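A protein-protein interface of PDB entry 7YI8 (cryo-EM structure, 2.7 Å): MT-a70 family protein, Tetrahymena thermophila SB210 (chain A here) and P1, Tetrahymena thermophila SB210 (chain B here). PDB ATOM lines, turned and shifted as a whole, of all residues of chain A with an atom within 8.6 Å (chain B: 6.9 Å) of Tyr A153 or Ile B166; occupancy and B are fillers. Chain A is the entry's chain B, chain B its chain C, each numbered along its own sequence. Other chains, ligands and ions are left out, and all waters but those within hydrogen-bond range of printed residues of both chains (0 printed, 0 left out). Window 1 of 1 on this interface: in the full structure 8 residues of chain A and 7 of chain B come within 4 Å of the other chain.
OE1 of Glu B157 sits close to OH of Tyr A153, 3.4 Å away.
ND2 of Asn B163 sits close to OE1 of Glu A160, at 3.2 Å.
NH2 of Arg A149 sits at hydrogen-bond distance from ND1 of His A152.
The side-chain hydroxyl (OH) of Tyr B171 is in hydrogen-bond range of the backbone carbonyl oxygen (O) of Leu B164, 2.7 Å away.
Among the printed residues, merely in contact across the chains: Ile A146 with Leu B170, Arg A149 with Glu B157, Ile A150 with Leu B170, Tyr A153 with Ile B166, Leu A156 with Asn B163, Phe A157 with Asn B163 and Phe A157 with Leu B164.
Of the printed residues of chain B, Ile A146 touches Leu B170 (3.6 Å).
Tyr A153 touches just these residues of chain B: Glu B157 (3.2 Å) and Ile B166 (3.7 Å).
Of the printed residues of chain B, Phe A157 touches Asn B163 (3.2 Å) and Leu B164 (3.8 Å).
Printed residues of chain A within 4 Å of Leu B164: Phe A157 (3.8 Å).
Printed residues of chain A within 4 Å of Ile B166: Tyr A153.
Of the printed residues of chain A, Leu B170 touches Ile A146 (3.6 Å) and Ile A150 (3.6 Å).
The nearest printed residue of chain B that does not touch Glu A160 is Thr B162 (6.9 Å).
Of the 16 printed residues of chain B, 5 touch a printed residue of chain A.
Of the 15 printed residues of chain A, 7 touch a printed residue of chain B.
Among the printed residues, 9 pairs touch across the chains.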
ATOM      1  N   ILE A 146     -25.464 -18.380  18.995  1.00  0.00           N
ATOM      2  CA  ILE A 146     -24.272 -19.187  19.214  1.00  0.00           C
ATOM      3  C   ILE A 146     -24.418 -20.020  20.482  1.00  0.00           C
ATOM      4  O   ILE A 146     -23.955 -21.165  20.531  1.00  0.00           O
ATOM      5  CB  ILE A 146     -23.009 -18.300  19.230  1.00  0.00           C
ATOM      6  CG1 ILE A 146     -21.794 -19.100  18.755  1.00  0.00           C
ATOM      7  CG2 ILE A 146     -22.750 -17.699  20.604  1.00  0.00           C
ATOM      8  CD1 ILE A 146     -21.887 -19.534  17.309  1.00  0.00           C
ATOM      9  N   GLU A 147     -25.088 -19.487  21.508  1.00  0.00           N
ATOM     10  CA  GLU A 147     -25.291 -20.248  22.736  1.00  0.00           C
ATOM     11  C   GLU A 147     -26.152 -21.478  22.482  1.00  0.00           C
ATOM     12  O   GLU A 147     -25.827 -22.581  22.937  1.00  0.00           O
ATOM     13  CB  GLU A 147     -25.924 -19.358  23.806  1.00  0.00           C
ATOM     14  CG  GLU A 147     -26.138 -20.052  25.141  1.00  0.00           C
ATOM     15  CD  GLU A 147     -24.837 -20.449  25.812  1.00  0.00           C
ATOM     16  OE1 GLU A 147     -23.803 -19.801  25.544  1.00  0.00           O
ATOM     17  OE2 GLU A 147     -24.848 -21.414  26.605  1.00  0.00           O
ATOM     18  N   LYS A 148     -27.251 -21.314  21.740  1.00  0.00           N
ATOM     19  CA  LYS A 148     -28.120 -22.459  21.478  1.00  0.00           C
ATOM     20  C   LYS A 148     -27.473 -23.453  20.517  1.00  0.00           C
ATOM     21  O   LYS A 148     -27.686 -24.664  20.649  1.00  0.00           O
ATOM     22  CB  LYS A 148     -29.480 -21.995  20.949  1.00  0.00           C
ATOM     23  CG  LYS A 148     -29.446 -21.194  19.663  1.00  0.00           C
ATOM     24  CD  LYS A 148     -30.851 -20.910  19.154  1.00  0.00           C
ATOM     25  CE  LYS A 148     -31.665 -20.129  20.173  1.00  0.00           C
ATOM     26  NZ  LYS A 148     -31.086 -18.784  20.440  1.00  0.00           N
ATOM     27  N   ARG A 149     -26.683 -22.970  19.554  1.00  0.00           N
ATOM     28  CA  ARG A 149     -25.941 -23.877  18.682  1.00  0.00           C
ATOM     29  C   ARG A 149     -24.951 -24.708  19.495  1.00  0.00           C
ATOM     30  O   ARG A 149     -24.861 -25.937  19.338  1.00  0.00           O
ATOM     31  CB  ARG A 149     -25.204 -23.068  17.615  1.00  0.00           C
ATOM     32  CG  ARG A 149     -24.362 -23.879  16.643  1.00  0.00           C
ATOM     33  CD  ARG A 149     -25.238 -24.678  15.687  1.00  0.00           C
ATOM     34  NE  ARG A 149     -25.672 -25.968  16.205  1.00  0.00           N
ATOM     35  CZ  ARG A 149     -26.563 -26.743  15.604  1.00  0.00           C
ATOM     36  NH1 ARG A 149     -27.142 -26.380  14.471  1.00  0.00           N
ATOM     37  NH2 ARG A 149     -26.879 -27.913  16.149  1.00  0.00           N
ATOM     38  N   ILE A 150     -24.212 -24.040  20.388  1.00  0.00           N
ATOM     39  CA  ILE A 150     -23.270 -24.723  21.266  1.00  0.00           C
ATOM     40  C   ILE A 150     -24.001 -25.727  22.139  1.00  0.00           C
ATOM     41  O   ILE A 150     -23.505 -26.831  22.387  1.00  0.00           O
ATOM     42  CB  ILE A 150     -22.491 -23.694  22.110  1.00  0.00           C
ATOM     43  CG1 ILE A 150     -21.342 -23.096  21.303  1.00  0.00           C
ATOM     44  CG2 ILE A 150     -21.962 -24.319  23.394  1.00  0.00           C
ATOM     45  CD1 ILE A 150     -20.543 -22.071  22.063  1.00  0.00           C
ATOM     46  N   LEU A 151     -25.195 -25.367  22.613  1.00  0.00           N
ATOM     47  CA  LEU A 151     -25.968 -26.294  23.431  1.00  0.00           C
ATOM     48  C   LEU A 151     -26.323 -27.544  22.637  1.00  0.00           C
ATOM     49  O   LEU A 151     -25.932 -28.656  23.012  1.00  0.00           O
ATOM     50  CB  LEU A 151     -27.219 -25.591  23.963  1.00  0.00           C
ATOM     51  CG  LEU A 151     -28.124 -26.279  24.991  1.00  0.00           C
ATOM     52  CD1 LEU A 151     -28.839 -25.228  25.821  1.00  0.00           C
ATOM     53  CD2 LEU A 151     -29.151 -27.186  24.322  1.00  0.00           C
ATOM     54  N   HIS A 152     -26.927 -27.368  21.460  1.00  0.00           N
ATOM     55  CA  HIS A 152     -27.351 -28.532  20.686  1.00  0.00           C
ATOM     56  C   HIS A 152     -26.163 -29.441  20.390  1.00  0.00           C
ATOM     57  O   HIS A 152     -26.266 -30.670  20.498  1.00  0.00           O
ATOM     58  CB  HIS A 152     -28.050 -28.095  19.398  1.00  0.00           C
ATOM     59  CG  HIS A 152     -28.661 -29.228  18.634  1.00  0.00           C
ATOM     60  ND1 HIS A 152     -29.108 -29.099  17.337  1.00  0.00           N
ATOM     61  CD2 HIS A 152     -28.914 -30.509  18.992  1.00  0.00           C
ATOM     62  CE1 HIS A 152     -29.598 -30.254  16.924  1.00  0.00           C
ATOM     63  NE2 HIS A 152     -29.494 -31.126  17.910  1.00  0.00           N
ATOM     64  N   TYR A 153     -25.005 -28.850  20.070  1.00  0.00           N
ATOM     65  CA  TYR A 153     -23.791 -29.661  19.959  1.00  0.00           C
ATOM     66  C   TYR A 153     -23.400 -30.316  21.282  1.00  0.00           C
ATOM     67  O   TYR A 153     -22.860 -31.426  21.279  1.00  0.00           O
ATOM     68  CB  TYR A 153     -22.634 -28.825  19.414  1.00  0.00           C
ATOM     69  CG  TYR A 153     -22.795 -28.423  17.968  1.00  0.00           C
ATOM     70  CD1 TYR A 153     -23.734 -29.047  17.159  1.00  0.00           C
ATOM     71  CD2 TYR A 153     -22.007 -27.428  17.408  1.00  0.00           C
ATOM     72  CE1 TYR A 153     -23.879 -28.698  15.834  1.00  0.00           C
ATOM     73  CE2 TYR A 153     -22.152 -27.066  16.083  1.00  0.00           C
ATOM     74  CZ  TYR A 153     -23.090 -27.704  15.303  1.00  0.00           C
ATOM     75  OH  TYR A 153     -23.243 -27.351  13.983  1.00  0.00           O
ATOM     76  N   LYS A 154     -23.656 -29.657  22.414  1.00  0.00           N
ATOM     77  CA  LYS A 154     -23.273 -30.230  23.702  1.00  0.00           C
ATOM     78  C   LYS A 154     -24.068 -31.494  24.005  1.00  0.00           C
ATOM     79  O   LYS A 154     -23.489 -32.537  24.322  1.00  0.00           O
ATOM     80  CB  LYS A 154     -23.459 -29.197  24.814  1.00  0.00           C
ATOM     81  CG  LYS A 154     -22.255 -28.300  25.035  1.00  0.00           C
ATOM     82  CD  LYS A 154     -22.513 -27.300  26.148  1.00  0.00           C
ATOM     83  CE  LYS A 154     -22.831 -28.003  27.455  1.00  0.00           C
ATOM     84  NZ  LYS A 154     -21.676 -28.797  27.957  1.00  0.00           N
ATOM     85  N   GLN A 155     -25.397 -31.426  23.901  1.00  0.00           N
ATOM     86  CA  GLN A 155     -26.183 -32.657  24.042  1.00  0.00           C
ATOM     87  C   GLN A 155     -25.905 -33.673  22.937  1.00  0.00           C
ATOM     88  O   GLN A 155     -25.971 -34.879  23.200  1.00  0.00           O
ATOM     89  CB  GLN A 155     -27.692 -32.396  24.169  1.00  0.00           C
ATOM     90  CG  GLN A 155     -28.198 -31.640  25.420  1.00  0.00           C
ATOM     91  CD  GLN A 155     -27.503 -30.352  25.753  1.00  0.00           C
ATOM     92  OE1 GLN A 155     -27.155 -29.585  24.879  1.00  0.00           O
ATOM     93  NE2 GLN A 155     -27.317 -30.096  27.042  1.00  0.00           N
ATOM     94  N   LEU A 156     -25.575 -33.240  21.717  1.00  0.00           N
ATOM     95  CA  LEU A 156     -25.181 -34.211  20.698  1.00  0.00           C
ATOM     96  C   LEU A 156     -23.945 -34.990  21.134  1.00  0.00           C
ATOM     97  O   LEU A 156     -23.908 -36.226  21.058  1.00  0.00           O
ATOM     98  CB  LEU A 156     -24.924 -33.500  19.368  1.00  0.00           C
ATOM     99  CG  LEU A 156     -26.080 -33.429  18.371  1.00  0.00           C
ATOM    100  CD1 LEU A 156     -25.662 -32.664  17.125  1.00  0.00           C
ATOM    101  CD2 LEU A 156     -26.567 -34.822  18.011  1.00  0.00           C
ATOM    102  N   PHE A 157     -22.927 -34.274  21.618  1.00  0.00           N
ATOM    103  CA  PHE A 157     -21.699 -34.919  22.070  1.00  0.00           C
ATOM    104  C   PHE A 157     -21.955 -35.797  23.286  1.00  0.00           C
ATOM    105  O   PHE A 157     -21.382 -36.885  23.406  1.00  0.00           O
ATOM    106  CB  PHE A 157     -20.634 -33.867  22.380  1.00  0.00           C
ATOM    107  CG  PHE A 157     -19.288 -34.446  22.716  1.00  0.00           C
ATOM    108  CD1 PHE A 157     -18.388 -34.761  21.715  1.00  0.00           C
ATOM    109  CD2 PHE A 157     -18.923 -34.676  24.032  1.00  0.00           C
ATOM    110  CE1 PHE A 157     -17.150 -35.296  22.018  1.00  0.00           C
ATOM    111  CE2 PHE A 157     -17.686 -35.208  24.341  1.00  0.00           C
ATOM    112  CZ  PHE A 157     -16.800 -35.518  23.332  1.00  0.00           C
ATOM    113  N   PHE A 158     -22.800 -35.333  24.208  1.00  0.00           N
ATOM    114  CA  PHE A 158     -23.134 -36.131  25.384  1.00  0.00           C
ATOM    115  C   PHE A 158     -23.824 -37.431  24.998  1.00  0.00           C
ATOM    116  O   PHE A 158     -23.505 -38.490  25.546  1.00  0.00           O
ATOM    117  CB  PHE A 158     -24.001 -35.320  26.348  1.00  0.00           C
ATOM    118  CG  PHE A 158     -23.297 -34.140  26.975  1.00  0.00           C
ATOM    119  CD1 PHE A 158     -22.057 -33.712  26.526  1.00  0.00           C
ATOM    120  CD2 PHE A 158     -23.904 -33.435  27.994  1.00  0.00           C
ATOM    121  CE1 PHE A 158     -21.431 -32.630  27.100  1.00  0.00           C
ATOM    122  CE2 PHE A 158     -23.282 -32.350  28.572  1.00  0.00           C
ATOM    123  CZ  PHE A 158     -22.045 -31.947  28.124  1.00  0.00           C
ATOM    124  N   LYS A 159     -24.767 -37.376  24.055  1.00  0.00           N
ATOM    125  CA  LYS A 159     -25.433 -38.596  23.606  1.00  0.00           C
ATOM    126  C   LYS A 159     -24.448 -39.545  22.933  1.00  0.00           C
ATOM    127  O   LYS A 159     -24.441 -40.755  23.207  1.00  0.00           O
ATOM    128  CB  LYS A 159     -26.579 -38.242  22.657  1.00  0.00           C
ATOM    129  CG  LYS A 159     -26.988 -39.368  21.722  1.00  0.00           C
ATOM    130  CD  LYS A 159     -27.698 -38.827  20.492  1.00  0.00           C
ATOM    131  CE  LYS A 159     -27.873 -39.907  19.437  1.00  0.00           C
ATOM    132  NZ  LYS A 159     -26.568 -40.384  18.905  1.00  0.00           N
ATOM    133  N   GLU A 160     -23.601 -39.012  22.047  1.00  0.00           N
ATOM    134  CA  GLU A 160     -22.642 -39.870  21.357  1.00  0.00           C
ATOM    135  C   GLU A 160     -21.661 -40.504  22.334  1.00  0.00           C
ATOM    136  O   GLU A 160     -21.339 -41.689  22.214  1.00  0.00           O
ATOM    137  CB  GLU A 160     -21.900 -39.082  20.279  1.00  0.00           C
ATOM    138  CG  GLU A 160     -22.800 -38.541  19.179  1.00  0.00           C
ATOM    139  CD  GLU A 160     -22.109 -38.494  17.829  1.00  0.00           C
ATOM    140  OE1 GLU A 160     -20.976 -39.008  17.721  1.00  0.00           O
ATOM    141  OE2 GLU A 160     -22.700 -37.942  16.878  1.00  0.00           O
ATOM    142  N   ILE B 156     -18.655 -22.897  10.040  1.00  0.00           N
ATOM    143  CA  ILE B 156     -17.985 -23.594  11.134  1.00  0.00           C
ATOM    144  C   ILE B 156     -18.271 -25.086  11.068  1.00  0.00           C
ATOM    145  O   ILE B 156     -17.374 -25.917  11.260  1.00  0.00           O
ATOM    146  CB  ILE B 156     -18.411 -22.997  12.488  1.00  0.00           C
ATOM    147  CG1 ILE B 156     -18.386 -21.465  12.439  1.00  0.00           C
ATOM    148  CG2 ILE B 156     -17.525 -23.525  13.605  1.00  0.00           C
ATOM    149  CD1 ILE B 156     -17.056 -20.878  12.013  1.00  0.00           C
ATOM    150  N   GLU B 157     -19.522 -25.452  10.799  1.00  0.00           N
ATOM    151  CA  GLU B 157     -19.940 -26.844  10.719  1.00  0.00           C
ATOM    152  C   GLU B 157     -20.135 -27.319   9.287  1.00  0.00           C
ATOM    153  O   GLU B 157     -20.743 -28.372   9.073  1.00  0.00           O
ATOM    154  CB  GLU B 157     -21.230 -27.048  11.514  1.00  0.00           C
ATOM    155  CG  GLU B 157     -22.311 -26.028  11.203  1.00  0.00           C
ATOM    156  CD  GLU B 157     -22.352 -24.900  12.215  1.00  0.00           C
ATOM    157  OE1 GLU B 157     -21.344 -24.700  12.923  1.00  0.00           O
ATOM    158  OE2 GLU B 157     -23.391 -24.215  12.302  1.00  0.00           O
ATOM    159  N   ASN B 158     -19.643 -26.564   8.301  1.00  0.00           N
ATOM    160  CA  ASN B 158     -19.812 -26.967   6.909  1.00  0.00           C
ATOM    161  C   ASN B 158     -19.107 -28.287   6.626  1.00  0.00           C
ATOM    162  O   ASN B 158     -19.660 -29.165   5.952  1.00  0.00           O
ATOM    163  CB  ASN B 158     -19.293 -25.870   5.980  1.00  0.00           C
ATOM    164  CG  ASN B 158     -20.403 -24.988   5.442  1.00  0.00           C
ATOM    165  OD1 ASN B 158     -21.585 -25.265   5.646  1.00  0.00           O
ATOM    166  ND2 ASN B 158     -20.027 -23.919   4.751  1.00  0.00           N
ATOM    167  N   GLU B 159     -17.889 -28.449   7.133  1.00  0.00           N
ATOM    168  CA  GLU B 159     -17.142 -29.684   6.966  1.00  0.00           C
ATOM    169  C   GLU B 159     -17.508 -30.677   8.063  1.00  0.00           C
ATOM    170  O   GLU B 159     -17.951 -30.296   9.150  1.00  0.00           O
ATOM    171  CB  GLU B 159     -15.637 -29.409   6.983  1.00  0.00           C
ATOM    172  CG  GLU B 159     -14.802 -30.470   6.284  1.00  0.00           C
ATOM    173  CD  GLU B 159     -13.321 -30.334   6.575  1.00  0.00           C
ATOM    174  OE1 GLU B 159     -12.912 -29.280   7.107  1.00  0.00           O
ATOM    175  OE2 GLU B 159     -12.564 -31.282   6.275  1.00  0.00           O
ATOM    176  N   LYS B 160     -17.324 -31.960   7.763  1.00  0.00           N
ATOM    177  CA  LYS B 160     -17.623 -33.033   8.709  1.00  0.00           C
ATOM    178  C   LYS B 160     -16.395 -33.273   9.580  1.00  0.00           C
ATOM    179  O   LYS B 160     -15.430 -33.911   9.154  1.00  0.00           O
ATOM    180  CB  LYS B 160     -18.043 -34.301   7.975  1.00  0.00           C
ATOM    181  CG  LYS B 160     -19.306 -34.145   7.144  1.00  0.00           C
ATOM    182  CD  LYS B 160     -20.518 -33.921   8.033  1.00  0.00           C
ATOM    183  CE  LYS B 160     -21.798 -33.843   7.218  1.00  0.00           C
ATOM    184  NZ  LYS B 160     -22.987 -33.580   8.075  1.00  0.00           N
ATOM    185  N   PHE B 161     -16.433 -32.755  10.802  1.00  0.00           N
ATOM    186  CA  PHE B 161     -15.386 -32.964  11.787  1.00  0.00           C
ATOM    187  C   PHE B 161     -15.797 -34.065  12.760  1.00  0.00           C
ATOM    188  O   PHE B 161     -16.956 -34.481  12.814  1.00  0.00           O
ATOM    189  CB  PHE B 161     -15.096 -31.667  12.547  1.00  0.00           C
ATOM    190  CG  PHE B 161     -14.624 -30.544  11.671  1.00  0.00           C
ATOM    191  CD1 PHE B 161     -13.385 -30.598  11.058  1.00  0.00           C
ATOM    192  CD2 PHE B 161     -15.422 -29.432  11.461  1.00  0.00           C
ATOM    193  CE1 PHE B 161     -12.950 -29.562  10.253  1.00  0.00           C
ATOM    194  CE2 PHE B 161     -14.994 -28.398  10.655  1.00  0.00           C
ATOM    195  CZ  PHE B 161     -13.756 -28.461  10.052  1.00  0.00           C
ATOM    196  N   THR B 162     -14.826 -34.538  13.536  1.00  0.00           N
ATOM    197  CA  THR B 162     -15.141 -35.484  14.592  1.00  0.00           C
ATOM    198  C   THR B 162     -15.926 -34.782  15.696  1.00  0.00           C
ATOM    199  O   THR B 162     -15.908 -33.555  15.821  1.00  0.00           O
ATOM    200  CB  THR B 162     -13.870 -36.121  15.158  1.00  0.00           C
ATOM    201  OG1 THR B 162     -14.223 -37.229  15.996  1.00  0.00           O
ATOM    202  CG2 THR B 162     -13.081 -35.116  15.978  1.00  0.00           C
ATOM    203  N   ASN B 163     -16.620 -35.584  16.508  1.00  0.00           N
ATOM    204  CA  ASN B 163     -17.590 -35.041  17.454  1.00  0.00           C
ATOM    205  C   ASN B 163     -16.972 -34.074  18.455  1.00  0.00           C
ATOM    206  O   ASN B 163     -17.695 -33.253  19.030  1.00  0.00           O
ATOM    207  CB  ASN B 163     -18.288 -36.174  18.202  1.00  0.00           C
ATOM    208  CG  ASN B 163     -19.686 -35.800  18.638  1.00  0.00           C
ATOM    209  OD1 ASN B 163     -20.289 -34.869  18.103  1.00  0.00           O
ATOM    210  ND2 ASN B 163     -20.207 -36.518  19.621  1.00  0.00           N
ATOM    211  N   LEU B 164     -15.665 -34.154  18.687  1.00  0.00           N
ATOM    212  CA  LEU B 164     -14.993 -33.176  19.534  1.00  0.00           C
ATOM    213  C   LEU B 164     -14.522 -31.962  18.746  1.00  0.00           C
ATOM    214  O   LEU B 164     -14.535 -30.843  19.273  1.00  0.00           O
ATOM    215  CB  LEU B 164     -13.806 -33.830  20.246  1.00  0.00           C
ATOM    216  CG  LEU B 164     -13.000 -32.989  21.239  1.00  0.00           C
ATOM    217  CD1 LEU B 164     -13.910 -32.127  22.104  1.00  0.00           C
ATOM    218  CD2 LEU B 164     -12.131 -33.891  22.100  1.00  0.00           C
ATOM    219  N   GLU B 165     -14.118 -32.157  17.491  1.00  0.00           N
ATOM    220  CA  GLU B 165     -13.648 -31.066  16.649  1.00  0.00           C
ATOM    221  C   GLU B 165     -14.786 -30.253  16.042  1.00  0.00           C
ATOM    222  O   GLU B 165     -14.517 -29.230  15.405  1.00  0.00           O
ATOM    223  CB  GLU B 165     -12.755 -31.619  15.534  1.00  0.00           C
ATOM    224  CG  GLU B 165     -11.830 -30.603  14.881  1.00  0.00           C
ATOM    225  CD  GLU B 165     -10.830 -31.251  13.944  1.00  0.00           C
ATOM    226  OE1 GLU B 165     -10.834 -32.495  13.836  1.00  0.00           O
ATOM    227  OE2 GLU B 165     -10.040 -30.517  13.315  1.00  0.00           O
ATOM    228  N   ILE B 166     -16.043 -30.673  16.228  1.00  0.00           N
ATOM    229  CA  ILE B 166     -17.178 -29.943  15.671  1.00  0.00           C
ATOM    230  C   ILE B 166     -17.185 -28.488  16.114  1.00  0.00           C
ATOM    231  O   ILE B 166     -17.785 -27.640  15.446  1.00  0.00           O
ATOM    232  CB  ILE B 166     -18.507 -30.633  16.042  1.00  0.00           C
ATOM    233  CG1 ILE B 166     -18.702 -30.654  17.558  1.00  0.00           C
ATOM    234  CG2 ILE B 166     -18.576 -32.033  15.456  1.00  0.00           C
ATOM    235  CD1 ILE B 166     -20.080 -31.104  17.986  1.00  0.00           C
ATOM    236  N   LEU B 167     -16.536 -28.176  17.231  1.00  0.00           N
ATOM    237  CA  LEU B 167     -16.281 -26.793  17.626  1.00  0.00           C
ATOM    238  C   LEU B 167     -14.941 -26.313  17.075  1.00  0.00           C
ATOM    239  O   LEU B 167     -14.096 -25.799  17.804  1.00  0.00           O
ATOM    240  CB  LEU B 167     -16.323 -26.667  19.144  1.00  0.00           C
ATOM    241  CG  LEU B 167     -17.576 -27.066  19.924  1.00  0.00           C
ATOM    242  CD1 LEU B 167     -17.566 -28.544  20.278  1.00  0.00           C
ATOM    243  CD2 LEU B 167     -17.693 -26.221  21.180  1.00  0.00           C
ATOM    244  N   THR B 168     -14.743 -26.481  15.763  1.00  0.00           N
ATOM    245  CA  THR B 168     -13.450 -26.162  15.162  1.00  0.00           C
ATOM    246  C   THR B 168     -13.134 -24.677  15.261  1.00  0.00           C
ATOM    247  O   THR B 168     -11.959 -24.290  15.252  1.00  0.00           O
ATOM    248  CB  THR B 168     -13.416 -26.616  13.701  1.00  0.00           C
ATOM    249  OG1 THR B 168     -12.092 -26.452  13.179  1.00  0.00           O
ATOM    250  CG2 THR B 168     -14.390 -25.800  12.862  1.00  0.00           C
ATOM    251  N   HIS B 169     -14.160 -23.832  15.353  1.00  0.00           N
ATOM    252  CA  HIS B 169     -13.975 -22.415  15.607  1.00  0.00           C
ATOM    253  C   HIS B 169     -14.599 -21.949  16.909  1.00  0.00           C
ATOM    254  O   HIS B 169     -14.198 -20.901  17.419  1.00  0.00           O
ATOM    255  CB  HIS B 169     -14.559 -21.573  14.461  1.00  0.00           C
ATOM    256  CG  HIS B 169     -13.703 -21.538  13.233  1.00  0.00           C
ATOM    257  ND1 HIS B 169     -13.848 -22.438  12.199  1.00  0.00           N
ATOM    258  CD2 HIS B 169     -12.697 -20.707  12.872  1.00  0.00           C
ATOM    259  CE1 HIS B 169     -12.965 -22.165  11.254  1.00  0.00           C
ATOM    260  NE2 HIS B 169     -12.255 -21.118  11.638  1.00  0.00           N
ATOM    261  N   LEU B 170     -15.543 -22.704  17.476  1.00  0.00           N
ATOM    262  CA  LEU B 170     -16.172 -22.294  18.725  1.00  0.00           C
ATOM    263  C   LEU B 170     -15.180 -22.266  19.879  1.00  0.00           C
ATOM    264  O   LEU B 170     -15.467 -21.652  20.914  1.00  0.00           O
ATOM    265  CB  LEU B 170     -17.333 -23.234  19.052  1.00  0.00           C
ATOM    266  CG  LEU B 170     -18.514 -23.190  18.081  1.00  0.00           C
ATOM    267  CD1 LEU B 170     -19.543 -24.257  18.419  1.00  0.00           C
ATOM    268  CD2 LEU B 170     -19.149 -21.812  18.085  1.00  0.00           C
ATOM    269  N   TYR B 171     -14.017 -22.903  19.712  1.00  0.00           N
ATOM    270  CA  TYR B 171     -13.016 -22.939  20.772  1.00  0.00           C
ATOM    271  C   TYR B 171     -12.623 -21.533  21.206  1.00  0.00           C
ATOM    272  O   TYR B 171     -12.640 -21.211  22.400  1.00  0.00           O
ATOM    273  CB  TYR B 171     -11.785 -23.716  20.302  1.00  0.00           C
ATOM    274  CG  TYR B 171     -11.976 -25.215  20.241  1.00  0.00           C
ATOM    275  CD1 TYR B 171     -13.143 -25.808  20.699  1.00  0.00           C
ATOM    276  CD2 TYR B 171     -10.984 -26.038  19.725  1.00  0.00           C
ATOM    277  CE1 TYR B 171     -13.317 -27.179  20.643  1.00  0.00           C
ATOM    278  CE2 TYR B 171     -11.151 -27.409  19.665  1.00  0.00           C
ATOM    279  CZ  TYR B 171     -12.319 -27.972  20.127  1.00  0.00           C
ATOM    280  OH  TYR B 171     -12.495 -29.335  20.071  1.00  0.00           O
